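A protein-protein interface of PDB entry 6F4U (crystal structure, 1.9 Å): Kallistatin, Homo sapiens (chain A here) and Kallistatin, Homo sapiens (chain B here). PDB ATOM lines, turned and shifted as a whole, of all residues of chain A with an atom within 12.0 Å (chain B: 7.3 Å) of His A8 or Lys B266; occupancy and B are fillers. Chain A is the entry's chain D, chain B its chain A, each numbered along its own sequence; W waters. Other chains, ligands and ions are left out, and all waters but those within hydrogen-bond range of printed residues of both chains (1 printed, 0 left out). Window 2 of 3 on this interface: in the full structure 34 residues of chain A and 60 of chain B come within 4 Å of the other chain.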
ATOM      1  N   ARG A   7      34.284   0.503 -24.680  1.00  0.00           N
ATOM      2  CA  ARG A   7      32.825   0.182 -24.768  1.00  0.00           C
ATOM      3  C   ARG A   7      32.207  -0.256 -23.410  1.00  0.00           C
ATOM      4  O   ARG A   7      31.008  -0.041 -23.185  1.00  0.00           O
ATOM      5  CB  ARG A   7      32.584  -0.881 -25.844  1.00  0.00           C
ATOM      6  CG  ARG A   7      31.121  -1.269 -26.032  1.00  0.00           C
ATOM      7  CD  ARG A   7      30.778  -1.695 -27.460  1.00  0.00           C
ATOM      8  NE  ARG A   7      29.341  -1.535 -27.728  1.00  0.00           N
ATOM      9  CZ  ARG A   7      28.734  -0.403 -28.088  1.00  0.00           C
ATOM     10  NH1 ARG A   7      29.396   0.738 -28.248  1.00  0.00           N
ATOM     11  NH2 ARG A   7      27.427  -0.408 -28.286  1.00  0.00           N
ATOM     12  N   HIS A   8      33.015  -0.862 -22.528  1.00  0.00           N
ATOM     13  CA  HIS A   8      32.571  -1.305 -21.191  1.00  0.00           C
ATOM     14  C   HIS A   8      33.068  -0.374 -20.089  1.00  0.00           C
ATOM     15  O   HIS A   8      33.454  -0.804 -19.006  1.00  0.00           O
ATOM     16  CB  HIS A   8      33.011  -2.762 -20.927  1.00  0.00           C
ATOM     17  CG  HIS A   8      32.482  -3.733 -21.933  1.00  0.00           C
ATOM     18  ND1 HIS A   8      31.131  -3.942 -22.125  1.00  0.00           N
ATOM     19  CD2 HIS A   8      33.116  -4.530 -22.825  1.00  0.00           C
ATOM     20  CE1 HIS A   8      30.957  -4.837 -23.081  1.00  0.00           C
ATOM     21  NE2 HIS A   8      32.146  -5.211 -23.522  1.00  0.00           N
ATOM     22  N   ILE A   9      33.019   0.924 -20.369  1.00  0.00           N
ATOM     23  CA  ILE A   9      33.474   1.946 -19.438  1.00  0.00           C
ATOM     24  C   ILE A   9      32.525   3.166 -19.465  1.00  0.00           C
ATOM     25  O   ILE A   9      32.049   3.565 -20.514  1.00  0.00           O
ATOM     26  CB  ILE A   9      34.937   2.360 -19.749  1.00  0.00           C
ATOM     27  CG1 ILE A   9      35.369   3.516 -18.845  1.00  0.00           C
ATOM     28  CG2 ILE A   9      35.086   2.771 -21.203  1.00  0.00           C
ATOM     29  CD1 ILE A   9      36.855   3.721 -18.771  1.00  0.00           C
ATOM     30  N   LEU A  10      32.246   3.732 -18.297  1.00  0.00           N
ATOM     31  CA  LEU A  10      31.583   5.020 -18.204  1.00  0.00           C
ATOM     32  C   LEU A  10      32.337   5.877 -17.237  1.00  0.00           C
ATOM     33  O   LEU A  10      32.622   5.442 -16.125  1.00  0.00           O
ATOM     34  CB  LEU A  10      30.123   4.879 -17.744  1.00  0.00           C
ATOM     35  CG  LEU A  10      29.159   4.244 -18.747  1.00  0.00           C
ATOM     36  CD1 LEU A  10      27.802   4.017 -18.103  1.00  0.00           C
ATOM     37  CD2 LEU A  10      29.006   5.094 -19.989  1.00  0.00           C
ATOM     38  N   ARG A  11      32.623   7.106 -17.655  1.00  0.00           N
ATOM     39  CA  ARG A  11      33.273   8.095 -16.820  1.00  0.00           C
ATOM     40  C   ARG A  11      32.401   9.285 -16.674  1.00  0.00           C
ATOM     41  O   ARG A  11      32.259  10.054 -17.622  1.00  0.00           O
ATOM     42  CB  ARG A  11      34.556   8.614 -17.468  1.00  0.00           C
ATOM     43  CG  ARG A  11      35.670   7.655 -17.536  1.00  0.00           C
ATOM     44  CD  ARG A  11      36.860   8.309 -18.259  1.00  0.00           C
ATOM     45  NE  ARG A  11      37.826   7.273 -18.571  1.00  0.00           N
ATOM     46  CZ  ARG A  11      38.672   6.748 -17.694  1.00  0.00           C
ATOM     47  NH1 ARG A  11      38.722   7.182 -16.434  1.00  0.00           N
ATOM     48  NH2 ARG A  11      39.479   5.780 -18.095  1.00  0.00           N
ATOM     49  N   PHE A  12      31.843   9.471 -15.479  1.00  0.00           N
ATOM     50  CA  PHE A  12      31.038  10.640 -15.184  1.00  0.00           C
ATOM     51  C   PHE A  12      31.917  11.792 -14.751  1.00  0.00           C
ATOM     52  O   PHE A  12      31.925  12.193 -13.581  1.00  0.00           O
ATOM     53  CB  PHE A  12      29.962  10.290 -14.156  1.00  0.00           C
ATOM     54  CG  PHE A  12      28.881   9.407 -14.721  1.00  0.00           C
ATOM     55  CD1 PHE A  12      29.051   8.026 -14.806  1.00  0.00           C
ATOM     56  CD2 PHE A  12      27.693   9.956 -15.157  1.00  0.00           C
ATOM     57  CE1 PHE A  12      28.042   7.215 -15.330  1.00  0.00           C
ATOM     58  CE2 PHE A  12      26.675   9.159 -15.686  1.00  0.00           C
ATOM     59  CZ  PHE A  12      26.867   7.783 -15.789  1.00  0.00           C
ATOM     60  N   ARG A  14      31.943  14.744 -16.730  1.00  0.00           N
ATOM     61  CA  ARG A  14      31.397  15.895 -17.444  1.00  0.00           C
ATOM     62  C   ARG A  14      29.927  15.952 -17.027  1.00  0.00           C
ATOM     63  O   ARG A  14      29.452  15.007 -16.426  1.00  0.00           O
ATOM     64  CB  ARG A  14      31.561  15.738 -18.960  1.00  0.00           C
ATOM     65  CG  ARG A  14      30.999  14.466 -19.562  1.00  0.00           C
ATOM     66  CD  ARG A  14      31.422  14.339 -21.018  1.00  0.00           C
ATOM     67  NE  ARG A  14      30.912  13.130 -21.674  1.00  0.00           N
ATOM     68  CZ  ARG A  14      31.342  11.889 -21.467  1.00  0.00           C
ATOM     69  NH1 ARG A  14      32.315  11.595 -20.575  1.00  0.00           N
ATOM     70  NH2 ARG A  14      30.773  10.898 -22.143  1.00  0.00           N
ATOM     71  N   ASP B 203      34.981  -1.661 -10.788  1.00  0.00           N
ATOM     72  CA  ASP B 203      35.179  -2.336 -12.069  1.00  0.00           C
ATOM     73  C   ASP B 203      34.958  -3.865 -12.079  1.00  0.00           C
ATOM     74  O   ASP B 203      35.159  -4.495 -13.116  1.00  0.00           O
ATOM     75  CB  ASP B 203      36.554  -1.971 -12.645  1.00  0.00           C
ATOM     76  CG  ASP B 203      37.710  -2.344 -11.721  1.00  0.00           C
ATOM     77  OD1 ASP B 203      37.505  -3.089 -10.745  1.00  0.00           O
ATOM     78  OD2 ASP B 203      38.830  -1.855 -11.955  1.00  0.00           O
ATOM     79  N   GLU B 205      31.927  -5.333 -11.122  1.00  0.00           N
ATOM     80  CA  GLU B 205      30.492  -5.648 -11.129  1.00  0.00           C
ATOM     81  C   GLU B 205      29.856  -5.546 -12.503  1.00  0.00           C
ATOM     82  O   GLU B 205      30.315  -4.782 -13.343  1.00  0.00           O
ATOM     83  CB  GLU B 205      29.755  -4.715 -10.167  1.00  0.00           C
ATOM     84  CG  GLU B 205      30.175  -4.880  -8.724  1.00  0.00           C
ATOM     85  CD  GLU B 205      29.878  -6.282  -8.231  1.00  0.00           C
ATOM     86  OE1 GLU B 205      28.700  -6.696  -8.314  1.00  0.00           O
ATOM     87  OE2 GLU B 205      30.814  -6.977  -7.815  1.00  0.00           O
ATOM     88  N   HIS B 206      28.797  -6.325 -12.726  1.00  0.00           N
ATOM     89  CA  HIS B 206      27.893  -6.093 -13.862  1.00  0.00           C
ATOM     90  C   HIS B 206      26.970  -4.930 -13.501  1.00  0.00           C
ATOM     91  O   HIS B 206      26.583  -4.773 -12.346  1.00  0.00           O
ATOM     92  CB  HIS B 206      27.046  -7.320 -14.199  1.00  0.00           C
ATOM     93  CG  HIS B 206      27.762  -8.348 -15.025  1.00  0.00           C
ATOM     94  ND1 HIS B 206      29.010  -8.832 -14.697  1.00  0.00           N
ATOM     95  CD2 HIS B 206      27.396  -8.990 -16.164  1.00  0.00           C
ATOM     96  CE1 HIS B 206      29.399  -9.702 -15.616  1.00  0.00           C
ATOM     97  NE2 HIS B 206      28.433  -9.825 -16.509  1.00  0.00           N
ATOM     98  N   HIS B 207      26.636  -4.131 -14.504  1.00  0.00           N
ATOM     99  CA  HIS B 207      25.718  -3.012 -14.365  1.00  0.00           C
ATOM    100  C   HIS B 207      24.779  -2.972 -15.542  1.00  0.00           C
ATOM    101  O   HIS B 207      25.126  -3.485 -16.615  1.00  0.00           O
ATOM    102  CB  HIS B 207      26.533  -1.725 -14.319  1.00  0.00           C
ATOM    103  CG  HIS B 207      27.062  -1.432 -12.967  1.00  0.00           C
ATOM    104  ND1 HIS B 207      26.273  -0.896 -11.978  1.00  0.00           N
ATOM    105  CD2 HIS B 207      28.275  -1.650 -12.411  1.00  0.00           C
ATOM    106  CE1 HIS B 207      26.985  -0.763 -10.874  1.00  0.00           C
ATOM    107  NE2 HIS B 207      28.194  -1.247 -11.099  1.00  0.00           N
ATOM    108  N   TRP B 208      23.630  -2.307 -15.349  1.00  0.00           N
ATOM    109  CA  TRP B 208      22.642  -2.072 -16.381  1.00  0.00           C
ATOM    110  C   TRP B 208      22.961  -0.746 -17.048  1.00  0.00           C
ATOM    111  O   TRP B 208      22.791   0.336 -16.439  1.00  0.00           O
ATOM    112  CB  TRP B 208      21.227  -2.072 -15.806  1.00  0.00           C
ATOM    113  CG  TRP B 208      20.832  -3.339 -15.150  1.00  0.00           C
ATOM    114  CD1 TRP B 208      20.981  -3.655 -13.834  1.00  0.00           C
ATOM    115  CD2 TRP B 208      20.212  -4.471 -15.763  1.00  0.00           C
ATOM    116  NE1 TRP B 208      20.502  -4.924 -13.591  1.00  0.00           N
ATOM    117  CE2 TRP B 208      20.026  -5.445 -14.759  1.00  0.00           C
ATOM    118  CE3 TRP B 208      19.794  -4.758 -17.071  1.00  0.00           C
ATOM    119  CZ2 TRP B 208      19.443  -6.696 -15.017  1.00  0.00           C
ATOM    120  CZ3 TRP B 208      19.198  -5.997 -17.321  1.00  0.00           C
ATOM    121  CH2 TRP B 208      19.023  -6.941 -16.296  1.00  0.00           C
ATOM    122  N   TYR B 209      23.439  -0.807 -18.294  1.00  0.00           N
ATOM    123  CA  TYR B 209      23.797   0.414 -19.023  1.00  0.00           C
ATOM    124  C   TYR B 209      23.744   0.254 -20.531  1.00  0.00           C
ATOM    125  O   TYR B 209      23.804  -0.864 -21.058  1.00  0.00           O
ATOM    126  CB  TYR B 209      25.165   0.958 -18.587  1.00  0.00           C
ATOM    127  CG  TYR B 209      26.339   0.109 -18.972  1.00  0.00           C
ATOM    128  CD1 TYR B 209      27.151   0.450 -20.056  1.00  0.00           C
ATOM    129  CD2 TYR B 209      26.631  -1.040 -18.273  1.00  0.00           C
ATOM    130  CE1 TYR B 209      28.217  -0.335 -20.426  1.00  0.00           C
ATOM    131  CE2 TYR B 209      27.706  -1.821 -18.610  1.00  0.00           C
ATOM    132  CZ  TYR B 209      28.488  -1.481 -19.695  1.00  0.00           C
ATOM    133  OH  TYR B 209      29.561  -2.278 -20.020  1.00  0.00           O
ATOM    134  N   HIS B 211      24.761   2.521 -24.443  1.00  0.00           N
ATOM    135  CA  HIS B 211      25.188   3.660 -25.236  1.00  0.00           C
ATOM    136  C   HIS B 211      24.092   3.828 -26.271  1.00  0.00           C
ATOM    137  O   HIS B 211      23.857   2.927 -27.059  1.00  0.00           O
ATOM    138  CB  HIS B 211      26.534   3.365 -25.899  1.00  0.00           C
ATOM    139  CG  HIS B 211      27.585   2.874 -24.949  1.00  0.00           C
ATOM    140  ND1 HIS B 211      28.004   3.607 -23.856  1.00  0.00           N
ATOM    141  CD2 HIS B 211      28.325   1.739 -24.944  1.00  0.00           C
ATOM    142  CE1 HIS B 211      28.951   2.939 -23.219  1.00  0.00           C
ATOM    143  NE2 HIS B 211      29.169   1.809 -23.865  1.00  0.00           N
ATOM    144  N   ARG B 262      18.563  -8.300 -20.515  1.00  0.00           N
ATOM    145  CA  ARG B 262      19.899  -8.642 -19.986  1.00  0.00           C
ATOM    146  C   ARG B 262      21.028  -8.503 -20.987  1.00  0.00           C
ATOM    147  O   ARG B 262      22.174  -8.500 -20.597  1.00  0.00           O
ATOM    148  CB  ARG B 262      19.955 -10.040 -19.257  1.00  0.00           C
ATOM    149  CG  ARG B 262      19.477 -11.205 -20.104  1.00  0.00           C
ATOM    150  CD  ARG B 262      20.184 -12.535 -19.916  1.00  0.00           C
ATOM    151  NE  ARG B 262      21.361 -12.607 -20.768  1.00  0.00           N
ATOM    152  CZ  ARG B 262      21.853 -13.688 -21.373  1.00  0.00           C
ATOM    153  NH1 ARG B 262      22.941 -13.520 -22.116  1.00  0.00           N
ATOM    154  NH2 ARG B 262      21.299 -14.912 -21.263  1.00  0.00           N
ATOM    155  N   ASN B 263      20.731  -8.366 -22.272  1.00  0.00           N
ATOM    156  CA  ASN B 263      21.715  -7.840 -23.237  1.00  0.00           C
ATOM    157  C   ASN B 263      22.490  -6.607 -22.707  1.00  0.00           C
ATOM    158  O   ASN B 263      23.670  -6.437 -23.014  1.00  0.00           O
ATOM    159  CB  ASN B 263      20.980  -7.454 -24.528  1.00  0.00           C
ATOM    160  CG  ASN B 263      21.884  -6.855 -25.545  1.00  0.00           C
ATOM    161  OD1 ASN B 263      21.750  -5.678 -25.893  1.00  0.00           O
ATOM    162  ND2 ASN B 263      22.853  -7.635 -25.990  1.00  0.00           N
ATOM    163  N   PHE B 264      21.832  -5.772 -21.891  1.00  0.00           N
ATOM    164  CA  PHE B 264      22.450  -4.566 -21.319  1.00  0.00           C
ATOM    165  C   PHE B 264      22.967  -4.696 -19.881  1.00  0.00           C
ATOM    166  O   PHE B 264      23.336  -3.694 -19.268  1.00  0.00           O
ATOM    167  CB  PHE B 264      21.450  -3.402 -21.431  1.00  0.00           C
ATOM    168  CG  PHE B 264      21.114  -3.052 -22.844  1.00  0.00           C
ATOM    169  CD1 PHE B 264      19.873  -3.329 -23.370  1.00  0.00           C
ATOM    170  CD2 PHE B 264      22.061  -2.465 -23.658  1.00  0.00           C
ATOM    171  CE1 PHE B 264      19.572  -3.018 -24.683  1.00  0.00           C
ATOM    172  CE2 PHE B 264      21.771  -2.148 -24.979  1.00  0.00           C
ATOM    173  CZ  PHE B 264      20.525  -2.411 -25.487  1.00  0.00           C
ATOM    174  N   TYR B 265      23.028  -5.924 -19.358  1.00  0.00           N
ATOM    175  CA  TYR B 265      23.642  -6.206 -18.081  1.00  0.00           C
ATOM    176  C   TYR B 265      25.014  -6.781 -18.357  1.00  0.00           C
ATOM    177  O   TYR B 265      25.140  -7.965 -18.730  1.00  0.00           O
ATOM    178  CB  TYR B 265      22.785  -7.186 -17.294  1.00  0.00           C
ATOM    179  CG  TYR B 265      23.205  -7.384 -15.868  1.00  0.00           C
ATOM    180  CD1 TYR B 265      23.199  -6.314 -14.963  1.00  0.00           C
ATOM    181  CD2 TYR B 265      23.563  -8.648 -15.392  1.00  0.00           C
ATOM    182  CE1 TYR B 265      23.589  -6.487 -13.636  1.00  0.00           C
ATOM    183  CE2 TYR B 265      23.950  -8.831 -14.065  1.00  0.00           C
ATOM    184  CZ  TYR B 265      23.936  -7.744 -13.195  1.00  0.00           C
ATOM    185  OH  TYR B 265      24.277  -7.898 -11.891  1.00  0.00           O
ATOM    186  N   LYS B 266      26.029  -5.939 -18.216  1.00  0.00           N
ATOM    187  CA  LYS B 266      27.390  -6.268 -18.604  1.00  0.00           C
ATOM    188  C   LYS B 266      28.370  -5.739 -17.581  1.00  0.00           C
ATOM    189  O   LYS B 266      28.088  -4.795 -16.861  1.00  0.00           O
ATOM    190  CB  LYS B 266      27.722  -5.648 -19.968  1.00  0.00           C
ATOM    191  CG  LYS B 266      26.779  -6.094 -21.089  1.00  0.00           C
ATOM    192  CD  LYS B 266      27.444  -6.110 -22.463  1.00  0.00           C
ATOM    193  CE  LYS B 266      26.899  -7.222 -23.377  1.00  0.00           C
ATOM    194  NZ  LYS B 266      27.379  -7.064 -24.779  1.00  0.00           N
ATOM    195  N   LYS B 267      29.551  -6.334 -17.554  1.00  0.00           N
ATOM    196  CA  LYS B 267      30.635  -5.834 -16.722  1.00  0.00           C
ATOM    197  C   LYS B 267      30.917  -4.385 -17.098  1.00  0.00           C
ATOM    198  O   LYS B 267      30.811  -4.004 -18.263  1.00  0.00           O
ATOM    199  CB  LYS B 267      31.896  -6.694 -16.888  1.00  0.00           C
ATOM    200  CG  LYS B 267      32.993  -6.368 -15.883  1.00  0.00           C
ATOM    201  CD  LYS B 267      34.142  -7.365 -15.992  1.00  0.00           C
ATOM    202  CE  LYS B 267      35.165  -7.171 -14.893  1.00  0.00           C
ATOM    203  NZ  LYS B 267      36.200  -8.252 -14.947  1.00  0.00           N
ATOM    204  N   LEU B 268      31.201  -3.559 -16.099  1.00  0.00           N
ATOM    205  CA  LEU B 268      31.397  -2.116 -16.335  1.00  0.00           C
ATOM    206  C   LEU B 268      32.535  -1.564 -15.491  1.00  0.00           C
ATOM    207  O   LEU B 268      32.598  -1.838 -14.302  1.00  0.00           O
ATOM    208  CB  LEU B 268      30.116  -1.339 -15.986  1.00  0.00           C
ATOM    209  CG  LEU B 268      30.153   0.197 -16.059  1.00  0.00           C
ATOM    210  CD1 LEU B 268      30.329   0.669 -17.483  1.00  0.00           C
ATOM    211  CD2 LEU B 268      28.896   0.793 -15.452  1.00  0.00           C
ATOM    212  N   GLU B 269      33.406  -0.770 -16.106  1.00  0.00           N
ATOM    213  CA  GLU B 269      34.334   0.091 -15.364  1.00  0.00           C
ATOM    214  C   GLU B 269      33.634   1.430 -15.171  1.00  0.00           C
ATOM    215  O   GLU B 269      33.422   2.145 -16.129  1.00  0.00           O
ATOM    216  CB  GLU B 269      35.650   0.275 -16.130  1.00  0.00           C
ATOM    217  CG  GLU B 269      36.699   1.124 -15.417  1.00  0.00           C
ATOM    218  CD  GLU B 269      37.885   1.452 -16.331  1.00  0.00           C
ATOM    219  OE1 GLU B 269      38.288   0.555 -17.088  1.00  0.00           O
ATOM    220  OE2 GLU B 269      38.399   2.592 -16.324  1.00  0.00           O
ATOM    221  N   LEU B 270      33.269   1.736 -13.926  1.00  0.00           N
ATOM    222  CA  LEU B 270      32.434   2.889 -13.593  1.00  0.00           C
ATOM    223  C   LEU B 270      33.224   3.891 -12.764  1.00  0.00           C
ATOM    224  O   LEU B 270      33.690   3.559 -11.679  1.00  0.00           O
ATOM    225  CB  LEU B 270      31.199   2.424 -12.807  1.00  0.00           C
ATOM    226  CG  LEU B 270      30.220   3.489 -12.308  1.00  0.00           C
ATOM    227  CD1 LEU B 270      29.756   4.409 -13.442  1.00  0.00           C
ATOM    228  CD2 LEU B 270      29.033   2.831 -11.639  1.00  0.00           C
HETATM  229  O   HOH W   1      34.454  -3.343 -17.908  1.00  0.00           O
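The side-chain carboxylate (OE2) of Glu B269 is in salt-bridge range of the guanidinium group (NH2) of Arg A11 (3.8 Å). N of Glu B269 sits at hydrogen-bond distance from O of His A8, at 2.9 Å. N of Leu A10 sits at hydrogen-bond distance from O of Glu B269 (2.9 Å). OH of Tyr B209 lies within hydrogen-bond range of ND1 of His A8 (3.1 Å). O of Arg A7 is in hydrogen-bond range of NE2 of His B211.
OH of Tyr B209 is in hydrogen-bond range of O of Lys B267. The backbone NH (N) of His B207 sits at hydrogen-bond distance from the backbone carbonyl oxygen (O) of Lys B266. The backbone NH (N) of Leu B268 lies within hydrogen-bond range of the backbone carbonyl oxygen (O) of Glu B205 (3.1 Å). The backbone carbonyl oxygen of Phe B264 is in hydrogen-bond range of the backbone NH of Tyr B209, 3.0 Å away. The backbone carbonyl oxygen (O) of Arg A11 lies within hydrogen-bond range of the guanidinium group (NH1) of Arg A14 (3.3 Å).
Among the printed residues, pairs that only touch across the chains: Ile A9 with Glu B269 (3.1 Å), Leu A10 with Leu B270 (3.6 Å), His A8 with Leu B268 (3.6 Å), His A8 with Lys B267 (3.7 Å), Leu A10 with Leu B268 (3.7 Å), His A8 with Lys B266 (3.8 Å), Phe A12 with Leu B270 (3.8 Å), Ile A9 with Leu B268 (3.9 Å), Leu A10 with His B211 (3.9 Å) and Arg A7 with Tyr B209 (3.9 Å).
Of chain B, only Tyr B209, Lys B266, Lys B267, Leu B268 and Glu B269 come within 4 Å of His A8. Of the printed residues of chain B, Leu A10 touches His B211 (3.9 Å), Leu B268 (3.7 Å), Glu B269 (2.9 Å) and Leu B270 (3.6 Å). Of the printed residues of chain B, Arg A11 touches Glu B269. No residue of chain A comes within 4 Å of His B207. No residue of chain A comes within 4 Å of Trp B208. No residue of chain A comes within 4 Å of Asn B263. No residue of chain A comes within 4 Å of Tyr B265. Lys B266 touches one residue of chain A. The nearest residue of chain B that does not touch His A8 is His B211 (4.9 Å). The nearest residue of chain A that does not touch Lys B266 is Arg A7 (6.6 Å). The nearest printed residue of chain B that does not touch Leu A10 is Tyr B209 (4.1 Å).
Among the printed residues, 15 pairs touch across the chains.
Water W1 bridges the backbone carbonyl oxygen of His A8 (2.9 Å) and the backbone NH of Glu B269 (3.3 Å).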
